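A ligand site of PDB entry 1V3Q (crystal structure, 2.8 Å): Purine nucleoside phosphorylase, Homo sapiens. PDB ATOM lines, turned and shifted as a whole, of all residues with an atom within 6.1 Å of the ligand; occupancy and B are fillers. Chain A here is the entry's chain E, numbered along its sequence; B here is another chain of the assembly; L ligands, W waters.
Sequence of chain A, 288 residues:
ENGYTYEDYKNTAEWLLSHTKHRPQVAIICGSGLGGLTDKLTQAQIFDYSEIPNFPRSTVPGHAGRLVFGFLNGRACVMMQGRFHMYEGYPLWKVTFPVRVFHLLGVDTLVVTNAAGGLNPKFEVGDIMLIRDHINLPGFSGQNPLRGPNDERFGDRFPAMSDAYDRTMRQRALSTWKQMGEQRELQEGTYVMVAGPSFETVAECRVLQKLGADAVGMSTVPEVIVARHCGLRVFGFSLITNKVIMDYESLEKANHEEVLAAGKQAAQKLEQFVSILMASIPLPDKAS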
ATOM      1  N   SER A  32      26.630  11.553  11.216  1.00  0.00           N
ATOM      2  CA  SER A  32      26.396  12.374  10.031  1.00  0.00           C
ATOM      3  C   SER A  32      27.624  13.104   9.530  1.00  0.00           C
ATOM      4  O   SER A  32      28.306  13.768  10.319  1.00  0.00           O
ATOM      5  CB  SER A  32      25.310  13.422  10.279  1.00  0.00           C
ATOM      6  OG  SER A  32      25.519  14.572   9.474  1.00  0.00           O
ATOM      7  N   HIS A  85      18.439   5.376  13.108  1.00  0.00           N
ATOM      8  CA  HIS A  85      17.990   6.230  14.198  1.00  0.00           C
ATOM      9  C   HIS A  85      16.606   5.814  14.643  1.00  0.00           C
ATOM     10  O   HIS A  85      15.818   5.252  13.870  1.00  0.00           O
ATOM     11  CB  HIS A  85      17.902   7.663  13.734  1.00  0.00           C
ATOM     12  CG  HIS A  85      19.164   8.204  13.166  1.00  0.00           C
ATOM     13  ND1 HIS A  85      19.647   7.813  11.948  1.00  0.00           N
ATOM     14  CD2 HIS A  85      19.991   9.161  13.631  1.00  0.00           C
ATOM     15  CE1 HIS A  85      20.731   8.513  11.670  1.00  0.00           C
ATOM     16  NE2 HIS A  85      20.963   9.343  12.668  1.00  0.00           N
ATOM     17  N   TYR A  87      14.252   7.900  15.363  1.00  0.00           N
ATOM     18  CA  TYR A  87      13.364   8.736  14.558  1.00  0.00           C
ATOM     19  C   TYR A  87      12.989   8.324  13.142  1.00  0.00           C
ATOM     20  O   TYR A  87      12.186   8.990  12.523  1.00  0.00           O
ATOM     21  CB  TYR A  87      13.827  10.182  14.530  1.00  0.00           C
ATOM     22  CG  TYR A  87      15.069  10.442  13.735  1.00  0.00           C
ATOM     23  CD1 TYR A  87      16.257  10.787  14.380  1.00  0.00           C
ATOM     24  CD2 TYR A  87      15.071  10.361  12.359  1.00  0.00           C
ATOM     25  CE1 TYR A  87      17.399  11.035  13.667  1.00  0.00           C
ATOM     26  CE2 TYR A  87      16.206  10.595  11.652  1.00  0.00           C
ATOM     27  CZ  TYR A  87      17.374  10.932  12.303  1.00  0.00           C
ATOM     28  OH  TYR A  87      18.536  11.097  11.595  1.00  0.00           O
ATOM     29  N   ALA A 115      26.996  13.782  15.261  1.00  0.00           N
ATOM     30  CA  ALA A 115      26.991  15.227  15.192  1.00  0.00           C
ATOM     31  C   ALA A 115      25.928  15.486  16.244  1.00  0.00           C
ATOM     32  O   ALA A 115      24.983  14.708  16.385  1.00  0.00           O
ATOM     33  CB  ALA A 115      26.509  15.681  13.853  1.00  0.00           C
ATOM     34  N   ALA A 116      26.084  16.564  17.005  1.00  0.00           N
ATOM     35  CA  ALA A 116      25.152  16.842  18.065  1.00  0.00           C
ATOM     36  C   ALA A 116      25.060  18.337  18.185  1.00  0.00           C
ATOM     37  O   ALA A 116      25.909  19.047  17.676  1.00  0.00           O
ATOM     38  CB  ALA A 116      25.694  16.264  19.344  1.00  0.00           C
ATOM     39  N   GLY A 117      24.034  18.808  18.880  1.00  0.00           N
ATOM     40  CA  GLY A 117      23.856  20.243  19.047  1.00  0.00           C
ATOM     41  C   GLY A 117      24.637  20.693  20.240  1.00  0.00           C
ATOM     42  O   GLY A 117      24.843  19.910  21.155  1.00  0.00           O
ATOM     43  N   GLY A 118      25.025  21.967  20.253  1.00  0.00           N
ATOM     44  CA  GLY A 118      25.804  22.510  21.349  1.00  0.00           C
ATOM     45  C   GLY A 118      24.916  23.144  22.390  1.00  0.00           C
ATOM     46  O   GLY A 118      24.133  24.026  22.080  1.00  0.00           O
ATOM     47  N   VAL A 194      17.842  12.529  22.662  1.00  0.00           N
ATOM     48  CA  VAL A 194      16.487  12.985  22.545  1.00  0.00           C
ATOM     49  C   VAL A 194      16.134  12.339  21.212  1.00  0.00           C
ATOM     50  O   VAL A 194      16.933  12.359  20.291  1.00  0.00           O
ATOM     51  CB  VAL A 194      16.484  14.493  22.466  1.00  0.00           C
ATOM     52  CG1 VAL A 194      15.454  14.979  21.481  1.00  0.00           C
ATOM     53  CG2 VAL A 194      16.255  15.068  23.837  1.00  0.00           C
ATOM     54  N   PRO A 197      12.431  13.635  15.533  1.00  0.00           N
ATOM     55  CA  PRO A 197      13.266  14.126  14.438  1.00  0.00           C
ATOM     56  C   PRO A 197      13.326  15.642  14.427  1.00  0.00           C
ATOM     57  O   PRO A 197      14.329  16.214  14.016  1.00  0.00           O
ATOM     58  CB  PRO A 197      12.599  13.531  13.205  1.00  0.00           C
ATOM     59  CG  PRO A 197      11.226  13.456  13.568  1.00  0.00           C
ATOM     60  CD  PRO A 197      11.199  13.018  15.012  1.00  0.00           C
ATOM     61  N   SER A 198      12.285  16.292  14.946  1.00  0.00           N
ATOM     62  CA  SER A 198      12.257  17.762  14.965  1.00  0.00           C
ATOM     63  C   SER A 198      13.355  18.299  15.869  1.00  0.00           C
ATOM     64  O   SER A 198      13.952  17.538  16.624  1.00  0.00           O
ATOM     65  CB  SER A 198      10.881  18.266  15.427  1.00  0.00           C
ATOM     66  OG  SER A 198      10.526  17.748  16.694  1.00  0.00           O
ATOM     67  N   PHE A 199      13.671  19.578  15.785  1.00  0.00           N
ATOM     68  CA  PHE A 199      14.713  20.148  16.633  1.00  0.00           C
ATOM     69  C   PHE A 199      14.155  20.805  17.868  1.00  0.00           C
ATOM     70  O   PHE A 199      13.069  21.354  17.849  1.00  0.00           O
ATOM     71  CB  PHE A 199      15.607  21.111  15.849  1.00  0.00           C
ATOM     72  CG  PHE A 199      16.700  20.424  15.062  1.00  0.00           C
ATOM     73  CD1 PHE A 199      16.839  19.056  15.082  1.00  0.00           C
ATOM     74  CD2 PHE A 199      17.587  21.159  14.304  1.00  0.00           C
ATOM     75  CE1 PHE A 199      17.833  18.436  14.351  1.00  0.00           C
ATOM     76  CE2 PHE A 199      18.580  20.554  13.573  1.00  0.00           C
ATOM     77  CZ  PHE A 199      18.703  19.185  13.605  1.00  0.00           C
ATOM     78  N   GLU A 200      14.927  20.761  18.951  1.00  0.00           N
ATOM     79  CA  GLU A 200      14.518  21.303  20.244  1.00  0.00           C
ATOM     80  C   GLU A 200      14.029  22.736  20.228  1.00  0.00           C
ATOM     81  O   GLU A 200      14.516  23.563  19.476  1.00  0.00           O
ATOM     82  CB  GLU A 200      15.654  21.195  21.278  1.00  0.00           C
ATOM     83  CG  GLU A 200      16.050  19.760  21.654  1.00  0.00           C
ATOM     84  CD  GLU A 200      16.687  19.006  20.503  1.00  0.00           C
ATOM     85  OE1 GLU A 200      16.509  17.769  20.422  1.00  0.00           O
ATOM     86  OE2 GLU A 200      17.359  19.642  19.668  1.00  0.00           O
ATOM     87  N   VAL A 216      23.413  17.675  22.566  1.00  0.00           N
ATOM     88  CA  VAL A 216      22.174  16.904  22.431  1.00  0.00           C
ATOM     89  C   VAL A 216      22.177  16.264  21.071  1.00  0.00           C
ATOM     90  O   VAL A 216      22.672  16.860  20.131  1.00  0.00           O
ATOM     91  CB  VAL A 216      20.904  17.763  22.537  1.00  0.00           C
ATOM     92  CG1 VAL A 216      20.964  18.987  21.621  1.00  0.00           C
ATOM     93  CG2 VAL A 216      19.699  16.932  22.158  1.00  0.00           C
ATOM     94  N   GLY A 217      21.617  15.064  20.966  1.00  0.00           N
ATOM     95  CA  GLY A 217      21.598  14.380  19.693  1.00  0.00           C
ATOM     96  C   GLY A 217      20.524  13.323  19.660  1.00  0.00           C
ATOM     97  O   GLY A 217      19.822  13.150  20.651  1.00  0.00           O
ATOM     98  N   MET A 218      20.431  12.563  18.584  1.00  0.00           N
ATOM     99  CA  MET A 218      19.381  11.558  18.453  1.00  0.00           C
ATOM    100  C   MET A 218      19.824  10.098  18.204  1.00  0.00           C
ATOM    101  O   MET A 218      19.096   9.338  17.566  1.00  0.00           O
ATOM    102  CB  MET A 218      18.415  11.991  17.333  1.00  0.00           C
ATOM    103  CG  MET A 218      17.882  13.443  17.411  1.00  0.00           C
ATOM    104  SD  MET A 218      17.069  14.022  15.902  1.00  0.00           S
ATOM    105  CE  MET A 218      17.110  15.682  16.211  1.00  0.00           C
ATOM    106  N   THR A 241      27.615  20.530  15.567  1.00  0.00           N
ATOM    107  CA  THR A 241      27.280  21.137  14.284  1.00  0.00           C
ATOM    108  C   THR A 241      26.509  22.438  14.417  1.00  0.00           C
ATOM    109  O   THR A 241      26.369  23.182  13.454  1.00  0.00           O
ATOM    110  CB  THR A 241      26.483  20.187  13.373  1.00  0.00           C
ATOM    111  OG1 THR A 241      25.263  19.781  14.022  1.00  0.00           O
ATOM    112  CG2 THR A 241      27.282  18.967  13.014  1.00  0.00           C
ATOM    113  N   ASN A 242      25.992  22.722  15.600  1.00  0.00           N
ATOM    114  CA  ASN A 242      25.261  23.960  15.750  1.00  0.00           C
ATOM    115  C   ASN A 242      24.992  24.229  17.198  1.00  0.00           C
ATOM    116  O   ASN A 242      24.799  23.305  17.971  1.00  0.00           O
ATOM    117  CB  ASN A 242      23.944  23.910  14.984  1.00  0.00           C
ATOM    118  CG  ASN A 242      23.032  22.795  15.467  1.00  0.00           C
ATOM    119  OD1 ASN A 242      23.216  21.639  15.107  1.00  0.00           O
ATOM    120  ND2 ASN A 242      22.050  23.145  16.281  1.00  0.00           N
ATOM    121  N   LYS A 243      25.037  25.499  17.571  1.00  0.00           N
ATOM    122  CA  LYS A 243      24.762  25.895  18.951  1.00  0.00           C
ATOM    123  C   LYS A 243      23.253  25.924  19.122  1.00  0.00           C
ATOM    124  O   LYS A 243      22.529  26.363  18.227  1.00  0.00           O
ATOM    125  CB  LYS A 243      25.387  27.250  19.271  1.00  0.00           C
ATOM    126  CG  LYS A 243      26.928  27.241  19.279  1.00  0.00           C
ATOM    127  CD  LYS A 243      27.496  28.253  20.271  1.00  0.00           C
ATOM    128  CE  LYS A 243      27.035  27.962  21.711  1.00  0.00           C
ATOM    129  NZ  LYS A 243      27.380  26.587  22.257  1.00  0.00           N
ATOM    130  N   VAL A 244      22.772  25.403  20.236  1.00  0.00           N
ATOM    131  CA  VAL A 244      21.350  25.349  20.502  1.00  0.00           C
ATOM    132  C   VAL A 244      20.881  26.662  21.108  1.00  0.00           C
ATOM    133  O   VAL A 244      21.528  27.211  21.994  1.00  0.00           O
ATOM    134  CB  VAL A 244      20.995  24.129  21.390  1.00  0.00           C
ATOM    135  CG1 VAL A 244      19.496  24.051  21.634  1.00  0.00           C
ATOM    136  CG2 VAL A 244      21.474  22.853  20.716  1.00  0.00           C
ATOM    137  N   ALA A 254      17.936  26.691  13.823  1.00  0.00           N
ATOM    138  CA  ALA A 254      18.587  25.379  13.611  1.00  0.00           C
ATOM    139  C   ALA A 254      18.079  24.756  12.322  1.00  0.00           C
ATOM    140  O   ALA A 254      16.865  24.637  12.125  1.00  0.00           O
ATOM    141  CB  ALA A 254      18.339  24.421  14.760  1.00  0.00           C
ATOM    142  N   ASN A 255      19.000  24.355  11.456  1.00  0.00           N
ATOM    143  CA  ASN A 255      18.648  23.751  10.175  1.00  0.00           C
ATOM    144  C   ASN A 255      19.647  22.666   9.842  1.00  0.00           C
ATOM    145  O   ASN A 255      20.745  22.633  10.410  1.00  0.00           O
ATOM    146  CB  ASN A 255      18.624  24.798   9.051  1.00  0.00           C
ATOM    147  CG  ASN A 255      19.938  25.561   8.936  1.00  0.00           C
ATOM    148  OD1 ASN A 255      20.897  25.080   8.352  1.00  0.00           O
ATOM    149  ND2 ASN A 255      19.961  26.765   9.476  1.00  0.00           N
ATOM    150  N   HIS A 256      19.282  21.759   8.945  1.00  0.00           N
ATOM    151  CA  HIS A 256      20.178  20.664   8.574  1.00  0.00           C
ATOM    152  C   HIS A 256      21.291  21.126   7.634  1.00  0.00           C
ATOM    153  O   HIS A 256      22.277  20.414   7.456  1.00  0.00           O
ATOM    154  CB  HIS A 256      19.413  19.484   7.960  1.00  0.00           C
ATOM    155  CG  HIS A 256      20.239  18.242   7.837  1.00  0.00           C
ATOM    156  ND1 HIS A 256      20.966  17.723   8.881  1.00  0.00           N
ATOM    157  CD2 HIS A 256      20.437  17.392   6.793  1.00  0.00           C
ATOM    158  CE1 HIS A 256      21.568  16.617   8.500  1.00  0.00           C
ATOM    159  NE2 HIS A 256      21.272  16.390   7.234  1.00  0.00           N
ATOM    160  N   GLU A 258      23.192  23.145   8.299  1.00  0.00           N
ATOM    161  CA  GLU A 258      24.295  23.250   9.249  1.00  0.00           C
ATOM    162  C   GLU A 258      25.148  21.965   9.178  1.00  0.00           C
ATOM    163  O   GLU A 258      26.166  21.850   9.867  1.00  0.00           O
ATOM    164  CB  GLU A 258      23.765  23.494  10.681  1.00  0.00           C
ATOM    165  CG  GLU A 258      23.095  24.876  10.905  1.00  0.00           C
ATOM    166  CD  GLU A 258      22.246  24.948  12.198  1.00  0.00           C
ATOM    167  OE1 GLU A 258      21.789  23.892  12.693  1.00  0.00           O
ATOM    168  OE2 GLU A 258      22.021  26.080  12.703  1.00  0.00           O
ATOM    169  N   VAL A 259      24.725  21.006   8.350  1.00  0.00           N
ATOM    170  CA  VAL A 259      25.492  19.776   8.148  1.00  0.00           C
ATOM    171  C   VAL A 259      26.772  20.150   7.393  1.00  0.00           C
ATOM    172  O   VAL A 259      27.726  19.371   7.354  1.00  0.00           O
ATOM    173  CB  VAL A 259      24.690  18.690   7.340  1.00  0.00           C
ATOM    174  CG1 VAL A 259      24.517  19.100   5.876  1.00  0.00           C
ATOM    175  CG2 VAL A 259      25.386  17.340   7.438  1.00  0.00           C
ATOM    176  N   PHE B 158      14.194  17.189   9.591  1.00  0.00           N
ATOM    177  CA  PHE B 158      14.444  17.825  10.869  1.00  0.00           C
ATOM    178  C   PHE B 158      13.856  19.246  10.971  1.00  0.00           C
ATOM    179  O   PHE B 158      14.585  20.222  10.820  1.00  0.00           O
ATOM    180  CB  PHE B 158      15.981  17.882  11.161  1.00  0.00           C
ATOM    181  CG  PHE B 158      16.707  16.559  10.982  1.00  0.00           C
ATOM    182  CD1 PHE B 158      16.664  15.575  11.970  1.00  0.00           C
ATOM    183  CD2 PHE B 158      17.387  16.267   9.800  1.00  0.00           C
ATOM    184  CE1 PHE B 158      17.284  14.326  11.771  1.00  0.00           C
ATOM    185  CE2 PHE B 158      18.015  15.032   9.596  1.00  0.00           C
ATOM    186  CZ  PHE B 158      17.955  14.062  10.579  1.00  0.00           C
HETATM  187  N1  LIG L   1      21.491  17.004  15.824  1.00  0.00           N
HETATM  188  C1  LIG L   1      20.666  17.456  16.821  1.00  0.00           C
HETATM  189  N2  LIG L   1      19.688  16.797  17.495  1.00  0.00           N
HETATM  190  C2  LIG L   1      19.089  17.577  18.380  1.00  0.00           C
HETATM  191  N3  LIG L   1      19.410  18.895  18.574  1.00  0.00           N
HETATM  192  C3  LIG L   1      20.407  19.591  17.894  1.00  0.00           C
HETATM  193  O1  LIG L   1      20.607  20.797  18.152  1.00  0.00           O
HETATM  194  C4  LIG L   1      21.055  18.770  16.955  1.00  0.00           C
HETATM  195  N4  LIG L   1      22.073  19.080  16.096  1.00  0.00           N
HETATM  196  C5  LIG L   1      22.341  17.967  15.382  1.00  0.00           C
HETATM  197  C6  LIG L   1      20.590  16.450  12.034  1.00  0.00           C
HETATM  198  O2  LIG L   1      21.820  16.906  11.385  1.00  0.00           O
HETATM  199  C7  LIG L   1      20.964  15.221  12.829  1.00  0.00           C
HETATM  200  O3  LIG L   1      21.965  15.647  13.797  1.00  0.00           O
HETATM  201  C8  LIG L   1      21.495  15.569  15.206  1.00  0.00           C
HETATM  202  C9  LIG L   1      20.116  14.877  15.104  1.00  0.00           C
HETATM  203  C10 LIG L   1      19.800  14.582  13.589  1.00  0.00           C
HETATM  204  O   HOH W   1      23.623  19.646  10.740  1.00  0.00           O
HETATM  205  O   HOH W   2      20.556  11.939  12.734  1.00  0.00           O
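O2 of the ligand sits at hydrogen-bond distance from ND1 of His 256 (2.8 Å).
The side-chain amide oxygen (OD1) of Asn 242 lies close to a nitrogen (N4) of the ligand, at 3.0 Å.
A nitrogen (N4) of the ligand lies within hydrogen-bond range of the backbone NH (N) of Gly 117, at 3.4 Å.
OE2 of Glu 200 lies within hydrogen-bond range of N3 of the ligand.
The side-chain amide oxygen of Asn 242 is in hydrogen-bond range of the side-chain hydroxyl of Thr 241 (3.0 Å).
O of Val 216 is in hydrogen-bond range of N of Gly 117, at 2.7 Å.
The backbone NH (N) of Val 244 lies within hydrogen-bond range of the backbone carbonyl oxygen (O) of Gly 118, at 2.7 Å.
N of Val 194 lies within hydrogen-bond range of O of Gly 217, 2.9 Å away.
The backbone NH of Thr 241 is in hydrogen-bond range of the backbone carbonyl oxygen of Ala 116 (3.1 Å).
O of Asn 242 sits at hydrogen-bond distance from N of Gly 118 (2.7 Å).
Ala 115 touches the ligand (O to C8, 3.8 Å).
Ala 116 touches the ligand (C to N4, 3.7 Å).
Phe 199 touches the ligand.
CG1 of Val 216 touches N3 of the ligand (3.4 Å).
Gly 217 touches the ligand.
Met 218 touches the ligand.
Thr 241 touches the ligand.
Val 244 touches the ligand (CG2 to O1, 3.4 Å).
CE1 of Phe 158 of chain B touches C10 of the ligand, 3.1 Å away.
Hydrophobic or aromatic side chains that line the ligand: Phe 199, Val 216, Met 218, Val 244, His 256 and Phe 158 of chain B.
13 residues have an atom within 4 Å of the ligand: Ala 115, Ala 116, Gly 117, Phe 199, Glu 200, Val 216, Gly 217, Met 218, Thr 241, Asn 242, Val 244, His 256 and Phe 158 of chain B.
Along chain A the residues within 4 Å of the ligand span positions 115 to 256.
Water W2 bridges the side-chain hydroxyl (OH) of Tyr 87 (2.5 Å) and a ring nitrogen (NE2) of His 85 (2.6 Å).
Water W1 lies within hydrogen-bond range of N of Val 259 (3.0 Å), O2 of the ligand (3.3 Å) and O of Glu 258 (3.5 Å).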
